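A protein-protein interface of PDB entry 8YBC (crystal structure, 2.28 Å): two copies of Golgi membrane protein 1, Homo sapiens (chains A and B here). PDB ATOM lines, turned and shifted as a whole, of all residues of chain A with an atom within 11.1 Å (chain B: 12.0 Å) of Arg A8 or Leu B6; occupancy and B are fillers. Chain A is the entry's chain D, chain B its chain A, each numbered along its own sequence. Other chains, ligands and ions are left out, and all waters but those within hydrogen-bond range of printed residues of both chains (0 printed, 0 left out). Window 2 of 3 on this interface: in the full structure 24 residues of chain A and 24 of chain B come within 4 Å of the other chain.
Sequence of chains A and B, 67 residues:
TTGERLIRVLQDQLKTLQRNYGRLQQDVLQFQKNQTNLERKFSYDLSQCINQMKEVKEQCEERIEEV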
ATOM      1  N   GLY A   3     -39.927   6.324 -25.959  1.00  0.00           N
ATOM      2  CA  GLY A   3     -39.563   7.208 -24.864  1.00  0.00           C
ATOM      3  C   GLY A   3     -38.159   7.768 -24.989  1.00  0.00           C
ATOM      4  O   GLY A   3     -37.859   8.498 -25.935  1.00  0.00           O
ATOM      5  N   GLU A   4     -37.283   7.433 -24.045  1.00  0.00           N
ATOM      6  CA  GLU A   4     -35.876   7.813 -24.132  1.00  0.00           C
ATOM      7  C   GLU A   4     -35.020   6.564 -24.298  1.00  0.00           C
ATOM      8  O   GLU A   4     -34.933   5.726 -23.390  1.00  0.00           O
ATOM      9  CB  GLU A   4     -35.439   8.635 -22.926  1.00  0.00           C
ATOM     10  CG  GLU A   4     -35.472  10.114 -23.247  1.00  0.00           C
ATOM     11  CD  GLU A   4     -34.638  10.434 -24.475  1.00  0.00           C
ATOM     12  OE1 GLU A   4     -35.082  11.284 -25.283  1.00  0.00           O
ATOM     13  OE2 GLU A   4     -33.542   9.834 -24.627  1.00  0.00           O
ATOM     14  N   ARG A   5     -34.387   6.459 -25.472  1.00  0.00           N
ATOM     15  CA  ARG A   5     -33.514   5.354 -25.833  1.00  0.00           C
ATOM     16  C   ARG A   5     -32.040   5.692 -25.632  1.00  0.00           C
ATOM     17  O   ARG A   5     -31.177   5.172 -26.361  1.00  0.00           O
ATOM     18  CB  ARG A   5     -33.777   4.948 -27.280  1.00  0.00           C
ATOM     19  CG  ARG A   5     -33.735   6.136 -28.240  1.00  0.00           C
ATOM     20  CD  ARG A   5     -33.154   5.769 -29.604  1.00  0.00           C
ATOM     21  NE  ARG A   5     -34.169   5.216 -30.501  1.00  0.00           N
ATOM     22  CZ  ARG A   5     -33.921   4.310 -31.442  1.00  0.00           C
ATOM     23  NH1 ARG A   5     -32.688   3.852 -31.613  1.00  0.00           N
ATOM     24  NH2 ARG A   5     -34.907   3.862 -32.211  1.00  0.00           N
ATOM     25  N   LEU A   6     -31.731   6.579 -24.677  1.00  0.00           N
ATOM     26  CA  LEU A   6     -30.363   6.692 -24.199  1.00  0.00           C
ATOM     27  C   LEU A   6     -29.814   5.325 -23.821  1.00  0.00           C
ATOM     28  O   LEU A   6     -28.617   5.066 -23.989  1.00  0.00           O
ATOM     29  CB  LEU A   6     -30.296   7.646 -23.000  1.00  0.00           C
ATOM     30  CG  LEU A   6     -28.924   7.786 -22.319  1.00  0.00           C
ATOM     31  CD1 LEU A   6     -27.860   8.195 -23.319  1.00  0.00           C
ATOM     32  CD2 LEU A   6     -28.987   8.781 -21.188  1.00  0.00           C
ATOM     33  N   ILE A   7     -30.687   4.431 -23.344  1.00  0.00           N
ATOM     34  CA  ILE A   7     -30.284   3.083 -22.955  1.00  0.00           C
ATOM     35  C   ILE A   7     -29.751   2.302 -24.150  1.00  0.00           C
ATOM     36  O   ILE A   7     -28.759   1.572 -24.037  1.00  0.00           O
ATOM     37  CB  ILE A   7     -31.466   2.361 -22.284  1.00  0.00           C
ATOM     38  CG1 ILE A   7     -31.900   3.144 -21.044  1.00  0.00           C
ATOM     39  CG2 ILE A   7     -31.093   0.915 -21.950  1.00  0.00           C
ATOM     40  CD1 ILE A   7     -33.152   2.629 -20.398  1.00  0.00           C
ATOM     41  N   ARG A   8     -30.399   2.435 -25.310  1.00  0.00           N
ATOM     42  CA  ARG A   8     -29.912   1.734 -26.492  1.00  0.00           C
ATOM     43  C   ARG A   8     -28.571   2.283 -26.966  1.00  0.00           C
ATOM     44  O   ARG A   8     -27.769   1.540 -27.546  1.00  0.00           O
ATOM     45  CB  ARG A   8     -30.945   1.805 -27.612  1.00  0.00           C
ATOM     46  CG  ARG A   8     -32.063   0.799 -27.452  1.00  0.00           C
ATOM     47  CD  ARG A   8     -32.895   0.676 -28.709  1.00  0.00           C
ATOM     48  NE  ARG A   8     -34.284   1.039 -28.445  1.00  0.00           N
ATOM     49  CZ  ARG A   8     -35.246   0.161 -28.179  1.00  0.00           C
ATOM     50  NH1 ARG A   8     -34.964  -1.135 -28.146  1.00  0.00           N
ATOM     51  NH2 ARG A   8     -36.487   0.574 -27.945  1.00  0.00           N
ATOM     52  N   VAL A   9     -28.319   3.576 -26.749  1.00  0.00           N
ATOM     53  CA  VAL A   9     -26.992   4.122 -27.016  1.00  0.00           C
ATOM     54  C   VAL A   9     -25.974   3.515 -26.055  1.00  0.00           C
ATOM     55  O   VAL A   9     -24.935   2.987 -26.473  1.00  0.00           O
ATOM     56  CB  VAL A   9     -27.019   5.656 -26.917  1.00  0.00           C
ATOM     57  CG1 VAL A   9     -25.641   6.214 -27.090  1.00  0.00           C
ATOM     58  CG2 VAL A   9     -27.948   6.222 -27.969  1.00  0.00           C
ATOM     59  N   LEU A  10     -26.292   3.545 -24.758  1.00  0.00           N
ATOM     60  CA  LEU A  10     -25.416   2.972 -23.743  1.00  0.00           C
ATOM     61  C   LEU A  10     -25.120   1.507 -24.024  1.00  0.00           C
ATOM     62  O   LEU A  10     -23.965   1.075 -23.933  1.00  0.00           O
ATOM     63  CB  LEU A  10     -26.044   3.127 -22.361  1.00  0.00           C
ATOM     64  CG  LEU A  10     -26.299   4.570 -21.942  1.00  0.00           C
ATOM     65  CD1 LEU A  10     -26.601   4.661 -20.442  1.00  0.00           C
ATOM     66  CD2 LEU A  10     -25.130   5.449 -22.337  1.00  0.00           C
ATOM     67  N   GLN A  11     -26.157   0.722 -24.345  1.00  0.00           N
ATOM     68  CA  GLN A  11     -25.938  -0.659 -24.771  1.00  0.00           C
ATOM     69  C   GLN A  11     -24.923  -0.751 -25.903  1.00  0.00           C
ATOM     70  O   GLN A  11     -24.097  -1.669 -25.927  1.00  0.00           O
ATOM     71  CB  GLN A  11     -27.246  -1.301 -25.220  1.00  0.00           C
ATOM     72  CG  GLN A  11     -27.910  -2.150 -24.175  1.00  0.00           C
ATOM     73  CD  GLN A  11     -29.325  -2.546 -24.561  1.00  0.00           C
ATOM     74  OE1 GLN A  11     -30.210  -2.607 -23.709  1.00  0.00           O
ATOM     75  NE2 GLN A  11     -29.543  -2.829 -25.840  1.00  0.00           N
ATOM     76  N   ASP A  12     -24.988   0.172 -26.868  1.00  0.00           N
ATOM     77  CA  ASP A  12     -24.009   0.143 -27.950  1.00  0.00           C
ATOM     78  C   ASP A  12     -22.612   0.459 -27.433  1.00  0.00           C
ATOM     79  O   ASP A  12     -21.630  -0.159 -27.859  1.00  0.00           O
ATOM     80  CB  ASP A  12     -24.382   1.133 -29.052  1.00  0.00           C
ATOM     81  CG  ASP A  12     -23.179   1.536 -29.898  1.00  0.00           C
ATOM     82  OD1 ASP A  12     -22.777   0.752 -30.797  1.00  0.00           O
ATOM     83  OD2 ASP A  12     -22.626   2.637 -29.654  1.00  0.00           O
ATOM     84  N   GLN A  13     -22.503   1.436 -26.533  1.00  0.00           N
ATOM     85  CA  GLN A  13     -21.189   1.810 -26.044  1.00  0.00           C
ATOM     86  C   GLN A  13     -20.587   0.708 -25.186  1.00  0.00           C
ATOM     87  O   GLN A  13     -19.375   0.487 -25.221  1.00  0.00           O
ATOM     88  CB  GLN A  13     -21.267   3.127 -25.280  1.00  0.00           C
ATOM     89  CG  GLN A  13     -21.353   4.320 -26.200  1.00  0.00           C
ATOM     90  CD  GLN A  13     -19.978   4.789 -26.674  1.00  0.00           C
ATOM     91  OE1 GLN A  13     -19.512   5.854 -26.278  1.00  0.00           O
ATOM     92  NE2 GLN A  13     -19.324   3.990 -27.522  1.00  0.00           N
ATOM     93  N   LEU A  14     -21.411  -0.019 -24.437  1.00  0.00           N
ATOM     94  CA  LEU A  14     -20.844  -1.067 -23.599  1.00  0.00           C
ATOM     95  C   LEU A  14     -20.330  -2.225 -24.442  1.00  0.00           C
ATOM     96  O   LEU A  14     -19.347  -2.876 -24.069  1.00  0.00           O
ATOM     97  CB  LEU A  14     -21.870  -1.541 -22.571  1.00  0.00           C
ATOM     98  CG  LEU A  14     -22.095  -0.572 -21.405  1.00  0.00           C
ATOM     99  CD1 LEU A  14     -23.084  -1.163 -20.423  1.00  0.00           C
ATOM    100  CD2 LEU A  14     -20.783  -0.249 -20.679  1.00  0.00           C
ATOM    101  N   LYS A  15     -20.954  -2.482 -25.588  1.00  0.00           N
ATOM    102  CA  LYS A  15     -20.433  -3.524 -26.460  1.00  0.00           C
ATOM    103  C   LYS A  15     -19.091  -3.119 -27.066  1.00  0.00           C
ATOM    104  O   LYS A  15     -18.215  -3.969 -27.262  1.00  0.00           O
ATOM    105  CB  LYS A  15     -21.454  -3.851 -27.540  1.00  0.00           C
ATOM    106  CG  LYS A  15     -22.556  -4.775 -27.047  1.00  0.00           C
ATOM    107  CD  LYS A  15     -23.822  -4.585 -27.846  1.00  0.00           C
ATOM    108  CE  LYS A  15     -24.950  -5.463 -27.348  1.00  0.00           C
ATOM    109  NZ  LYS A  15     -26.125  -5.283 -28.248  1.00  0.00           N
ATOM    110  N   THR A  16     -18.912  -1.829 -27.367  1.00  0.00           N
ATOM    111  CA  THR A  16     -17.607  -1.328 -27.799  1.00  0.00           C
ATOM    112  C   THR A  16     -16.578  -1.451 -26.678  1.00  0.00           C
ATOM    113  O   THR A  16     -15.481  -1.985 -26.879  1.00  0.00           O
ATOM    114  CB  THR A  16     -17.743   0.127 -28.255  1.00  0.00           C
ATOM    115  OG1 THR A  16     -18.629   0.189 -29.378  1.00  0.00           O
ATOM    116  CG2 THR A  16     -16.394   0.716 -28.642  1.00  0.00           C
ATOM    117  N   THR B   1     -42.134  -1.782 -17.554  1.00  0.00           N
ATOM    118  CA  THR B   1     -41.325  -2.719 -18.322  1.00  0.00           C
ATOM    119  C   THR B   1     -41.024  -2.126 -19.707  1.00  0.00           C
ATOM    120  O   THR B   1     -41.301  -0.949 -19.935  1.00  0.00           O
ATOM    121  CB  THR B   1     -42.021  -4.095 -18.442  1.00  0.00           C
ATOM    122  OG1 THR B   1     -43.344  -3.925 -18.953  1.00  0.00           O
ATOM    123  CG2 THR B   1     -42.104  -4.763 -17.064  1.00  0.00           C
ATOM    124  N   THR B   2     -40.435  -2.941 -20.599  1.00  0.00           N
ATOM    125  CA  THR B   2     -39.970  -2.572 -21.944  1.00  0.00           C
ATOM    126  C   THR B   2     -38.758  -1.642 -21.896  1.00  0.00           C
ATOM    127  O   THR B   2     -37.820  -1.798 -22.685  1.00  0.00           O
ATOM    128  CB  THR B   2     -41.095  -1.942 -22.779  1.00  0.00           C
ATOM    129  OG1 THR B   2     -42.155  -2.892 -22.952  1.00  0.00           O
ATOM    130  CG2 THR B   2     -40.585  -1.524 -24.157  1.00  0.00           C
ATOM    131  N   GLY B   3     -38.769  -0.672 -20.980  1.00  0.00           N
ATOM    132  CA  GLY B   3     -37.603   0.134 -20.679  1.00  0.00           C
ATOM    133  C   GLY B   3     -36.860  -0.421 -19.479  1.00  0.00           C
ATOM    134  O   GLY B   3     -35.644  -0.243 -19.351  1.00  0.00           O
ATOM    135  N   GLU B   4     -37.592  -1.095 -18.586  1.00  0.00           N
ATOM    136  CA  GLU B   4     -36.950  -1.879 -17.536  1.00  0.00           C
ATOM    137  C   GLU B   4     -36.210  -3.080 -18.111  1.00  0.00           C
ATOM    138  O   GLU B   4     -35.183  -3.491 -17.564  1.00  0.00           O
ATOM    139  CB  GLU B   4     -37.991  -2.341 -16.516  1.00  0.00           C
ATOM    140  CG  GLU B   4     -37.447  -2.617 -15.123  1.00  0.00           C
ATOM    141  CD  GLU B   4     -38.543  -2.622 -14.061  1.00  0.00           C
ATOM    142  OE1 GLU B   4     -39.626  -2.030 -14.296  1.00  0.00           O
ATOM    143  OE2 GLU B   4     -38.329  -3.239 -12.995  1.00  0.00           O
ATOM    144  N   ARG B   5     -36.706  -3.653 -19.209  1.00  0.00           N
ATOM    145  CA  ARG B   5     -36.035  -4.806 -19.796  1.00  0.00           C
ATOM    146  C   ARG B   5     -34.680  -4.413 -20.370  1.00  0.00           C
ATOM    147  O   ARG B   5     -33.667  -5.076 -20.105  1.00  0.00           O
ATOM    148  CB  ARG B   5     -36.903  -5.445 -20.874  1.00  0.00           C
ATOM    149  CG  ARG B   5     -36.107  -6.258 -21.889  1.00  0.00           C
ATOM    150  CD  ARG B   5     -37.007  -6.788 -22.980  1.00  0.00           C
ATOM    151  NE  ARG B   5     -37.879  -5.729 -23.471  1.00  0.00           N
ATOM    152  CZ  ARG B   5     -38.011  -5.387 -24.749  1.00  0.00           C
ATOM    153  NH1 ARG B   5     -37.326  -6.030 -25.688  1.00  0.00           N
ATOM    154  NH2 ARG B   5     -38.841  -4.402 -25.083  1.00  0.00           N
ATOM    155  N   LEU B   6     -34.650  -3.334 -21.163  1.00  0.00           N
ATOM    156  CA  LEU B   6     -33.396  -2.821 -21.707  1.00  0.00           C
ATOM    157  C   LEU B   6     -32.405  -2.457 -20.606  1.00  0.00           C
ATOM    158  O   LEU B   6     -31.211  -2.769 -20.708  1.00  0.00           O
ATOM    159  CB  LEU B   6     -33.681  -1.611 -22.591  1.00  0.00           C
ATOM    160  CG  LEU B   6     -34.339  -1.952 -23.922  1.00  0.00           C
ATOM    161  CD1 LEU B   6     -34.840  -0.680 -24.574  1.00  0.00           C
ATOM    162  CD2 LEU B   6     -33.341  -2.689 -24.824  1.00  0.00           C
ATOM    163  N   ILE B   7     -32.884  -1.799 -19.547  1.00  0.00           N
ATOM    164  CA  ILE B   7     -32.025  -1.435 -18.424  1.00  0.00           C
ATOM    165  C   ILE B   7     -31.424  -2.673 -17.768  1.00  0.00           C
ATOM    166  O   ILE B   7     -30.311  -2.614 -17.228  1.00  0.00           O
ATOM    167  CB  ILE B   7     -32.805  -0.574 -17.407  1.00  0.00           C
ATOM    168  CG1 ILE B   7     -31.865   0.372 -16.682  1.00  0.00           C
ATOM    169  CG2 ILE B   7     -33.432  -1.427 -16.339  1.00  0.00           C
ATOM    170  CD1 ILE B   7     -31.378   1.491 -17.541  1.00  0.00           C
ATOM    171  N   ARG B   8     -32.128  -3.812 -17.823  1.00  0.00           N
ATOM    172  CA  ARG B   8     -31.626  -5.037 -17.204  1.00  0.00           C
ATOM    173  C   ARG B   8     -30.531  -5.665 -18.046  1.00  0.00           C
ATOM    174  O   ARG B   8     -29.553  -6.184 -17.499  1.00  0.00           O
ATOM    175  CB  ARG B   8     -32.762  -6.040 -16.968  1.00  0.00           C
ATOM    176  CG  ARG B   8     -33.563  -5.749 -15.695  1.00  0.00           C
ATOM    177  CD  ARG B   8     -34.951  -6.393 -15.678  1.00  0.00           C
ATOM    178  NE  ARG B   8     -35.655  -6.080 -14.431  1.00  0.00           N
ATOM    179  CZ  ARG B   8     -36.692  -6.767 -13.948  1.00  0.00           C
ATOM    180  NH1 ARG B   8     -37.150  -7.829 -14.601  1.00  0.00           N
ATOM    181  NH2 ARG B   8     -37.265  -6.396 -12.804  1.00  0.00           N
ATOM    182  N   VAL B   9     -30.671  -5.619 -19.370  1.00  0.00           N
ATOM    183  CA  VAL B   9     -29.585  -6.059 -20.238  1.00  0.00           C
ATOM    184  C   VAL B   9     -28.356  -5.178 -20.042  1.00  0.00           C
ATOM    185  O   VAL B   9     -27.224  -5.666 -20.045  1.00  0.00           O
ATOM    186  CB  VAL B   9     -30.038  -6.069 -21.708  1.00  0.00           C
ATOM    187  CG1 VAL B   9     -28.977  -6.735 -22.580  1.00  0.00           C
ATOM    188  CG2 VAL B   9     -31.391  -6.750 -21.852  1.00  0.00           C
ATOM    189  N   LEU B  10     -28.561  -3.866 -19.889  1.00  0.00           N
ATOM    190  CA  LEU B  10     -27.449  -2.943 -19.672  1.00  0.00           C
ATOM    191  C   LEU B  10     -26.741  -3.240 -18.365  1.00  0.00           C
ATOM    192  O   LEU B  10     -25.508  -3.206 -18.288  1.00  0.00           O
ATOM    193  CB  LEU B  10     -27.956  -1.501 -19.664  1.00  0.00           C
ATOM    194  CG  LEU B  10     -26.859  -0.450 -19.778  1.00  0.00           C
ATOM    195  CD1 LEU B  10     -26.399  -0.441 -21.213  1.00  0.00           C
ATOM    196  CD2 LEU B  10     -27.325   0.945 -19.347  1.00  0.00           C
ATOM    197  N   GLN B  11     -27.510  -3.508 -17.316  1.00  0.00           N
ATOM    198  CA  GLN B  11     -26.904  -3.903 -16.056  1.00  0.00           C
ATOM    199  C   GLN B  11     -26.119  -5.189 -16.222  1.00  0.00           C
ATOM    200  O   GLN B  11     -25.067  -5.366 -15.588  1.00  0.00           O
ATOM    201  CB  GLN B  11     -27.985  -4.063 -14.990  1.00  0.00           C
ATOM    202  CG  GLN B  11     -28.579  -2.752 -14.535  1.00  0.00           C
ATOM    203  CD  GLN B  11     -29.950  -2.932 -13.909  1.00  0.00           C
ATOM    204  OE1 GLN B  11     -30.588  -3.970 -14.071  1.00  0.00           O
ATOM    205  NE2 GLN B  11     -30.404  -1.921 -13.187  1.00  0.00           N
ATOM    206  N   ASP B  12     -26.614  -6.097 -17.077  1.00  0.00           N
ATOM    207  CA  ASP B  12     -25.934  -7.371 -17.294  1.00  0.00           C
ATOM    208  C   ASP B  12     -24.603  -7.170 -18.003  1.00  0.00           C
ATOM    209  O   ASP B  12     -23.586  -7.741 -17.595  1.00  0.00           O
ATOM    210  CB  ASP B  12     -26.813  -8.336 -18.090  1.00  0.00           C
ATOM    211  CG  ASP B  12     -27.857  -9.046 -17.226  1.00  0.00           C
ATOM    212  OD1 ASP B  12     -27.952  -8.775 -16.002  1.00  0.00           O
ATOM    213  OD2 ASP B  12     -28.593  -9.891 -17.781  1.00  0.00           O
ATOM    214  N   GLN B  13     -24.599  -6.366 -19.079  1.00  0.00           N
ATOM    215  CA  GLN B  13     -23.367  -6.066 -19.812  1.00  0.00           C
ATOM    216  C   GLN B  13     -22.330  -5.416 -18.908  1.00  0.00           C
ATOM    217  O   GLN B  13     -21.135  -5.706 -19.011  1.00  0.00           O
ATOM    218  CB  GLN B  13     -23.658  -5.133 -20.995  1.00  0.00           C
ATOM    219  CG  GLN B  13     -24.200  -5.778 -22.274  1.00  0.00           C
ATOM    220  CD  GLN B  13     -24.836  -4.748 -23.200  1.00  0.00           C
ATOM    221  OE1 GLN B  13     -26.026  -4.437 -23.090  1.00  0.00           O
ATOM    222  NE2 GLN B  13     -24.036  -4.189 -24.091  1.00  0.00           N
ATOM    223  N   LEU B  14     -22.773  -4.522 -18.026  1.00  0.00           N
ATOM    224  CA  LEU B  14     -21.862  -3.825 -17.129  1.00  0.00           C
ATOM    225  C   LEU B  14     -21.252  -4.763 -16.088  1.00  0.00           C
ATOM    226  O   LEU B  14     -20.045  -4.694 -15.813  1.00  0.00           O
ATOM    227  CB  LEU B  14     -22.603  -2.686 -16.442  1.00  0.00           C
ATOM    228  CG  LEU B  14     -21.728  -1.929 -15.463  1.00  0.00           C
ATOM    229  CD1 LEU B  14     -20.677  -1.160 -16.280  1.00  0.00           C
ATOM    230  CD2 LEU B  14     -22.589  -1.024 -14.537  1.00  0.00           C
ATOM    231  N   LYS B  15     -22.059  -5.637 -15.482  1.00  0.00           N
ATOM    232  CA  LYS B  15     -21.480  -6.521 -14.485  1.00  0.00           C
ATOM    233  C   LYS B  15     -20.642  -7.635 -15.110  1.00  0.00           C
ATOM    234  O   LYS B  15     -19.716  -8.133 -14.461  1.00  0.00           O
ATOM    235  CB  LYS B  15     -22.555  -7.106 -13.567  1.00  0.00           C
ATOM    236  CG  LYS B  15     -21.963  -7.611 -12.246  1.00  0.00           C
ATOM    237  CD  LYS B  15     -22.776  -8.730 -11.606  1.00  0.00           C
ATOM    238  CE  LYS B  15     -22.715  -8.656 -10.078  1.00  0.00           C
ATOM    239  NZ  LYS B  15     -23.901  -9.296  -9.438  1.00  0.00           N
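NE2 of Gln B13 sits at hydrogen-bond distance from O of Gln A11 (3.1 Å).
The side-chain amide oxygen (OE1) of Gln A11 lies close to the backbone carbonyl oxygen (O) of Leu B6, at 3.2 Å.
The backbone carbonyl oxygen (O) of Ile B7 lies close to the side-chain amide oxygen (OE1) of Gln B11, at 3.4 Å.
O of Val B9 sits close to OE1 of Gln B13 (3.5 Å).
Ile A7 touches Gly B3 (CD1 to O, 3.9 Å).
Leu B6 touches Ile A7.
Ile A7 touches Ile B7 (CD1 to CD1, 3.6 Å).
NH1 of Arg A8 touches CD1 of Leu B6, at 3.6 Å.
CD1 of Leu B10 touches C of Leu A10 (3.7 Å).
CD1 of Leu B10 touches N of Gln A11, 3.3 Å away.
Leu B10 touches Leu A14.
Leu A14 touches Gln B13 (CB to NE2, 3.7 Å).
NE2 of Gln B13 touches CG of Lys A15 (3.4 Å).
Arg A8 touches just one residue of chain B: Leu B6.
Of chain A, only Ile A7, Arg A8 and Gln A11 come within 4 Å of Leu B6.
No residue of chain B comes within 4 Å of Arg A5.
No residue of chain B comes within 4 Å of Leu A6.
No residue of chain B comes within 4 Å of Val A9.
Of chain B, only Leu B10 comes within 4 Å of Leu A10.
Asp A12 touches none of the printed residues of chain B.
Of chain A, only Ile A7 comes within 4 Å of Gly B3.
No residue of chain A comes within 4 Å of Arg B5.
Printed residues of chain B within 4 Å of Lys A15: Gln B13.
Printed residues of chain B within 4 Å of Gln A11: Leu B6, Leu B10 and Gln B13.
Printed residues of chain B within 4 Å of Leu A14: Leu B10 and Gln B13.
Lys B15 touches none of the printed residues of chain A.
Thr B1 touches none of the printed residues of chain A.
The nearest printed residue of chain B that does not touch Lys A15 is Val B9 (6.4 Å).
Hydrophobic or aromatic side chains of chain A that line the printed part of chain B: Ile A7, Leu A10 and Leu A14.
Among the printed residues, 11 pairs touch across the chains.
Leu A10 touches its own counterpart, Leu B10.
Gln A11 touches Leu B10, but with the chains exchanged Leu A10 does not touch Gln B11 (8.5 Å).
Leu A14 touches Leu B10, but with the chains exchanged Leu A10 does not touch Leu B14 (8.2 Å).
Lys A15 touches Gln B13, but with the chains exchanged Gln A13 does not touch Lys B15 (11.7 Å).
13 positions are printed for both chains.
Of the 11 pairs that touch across the chains among the printed residues, 2 have their exchanged pair printed and touching as well.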
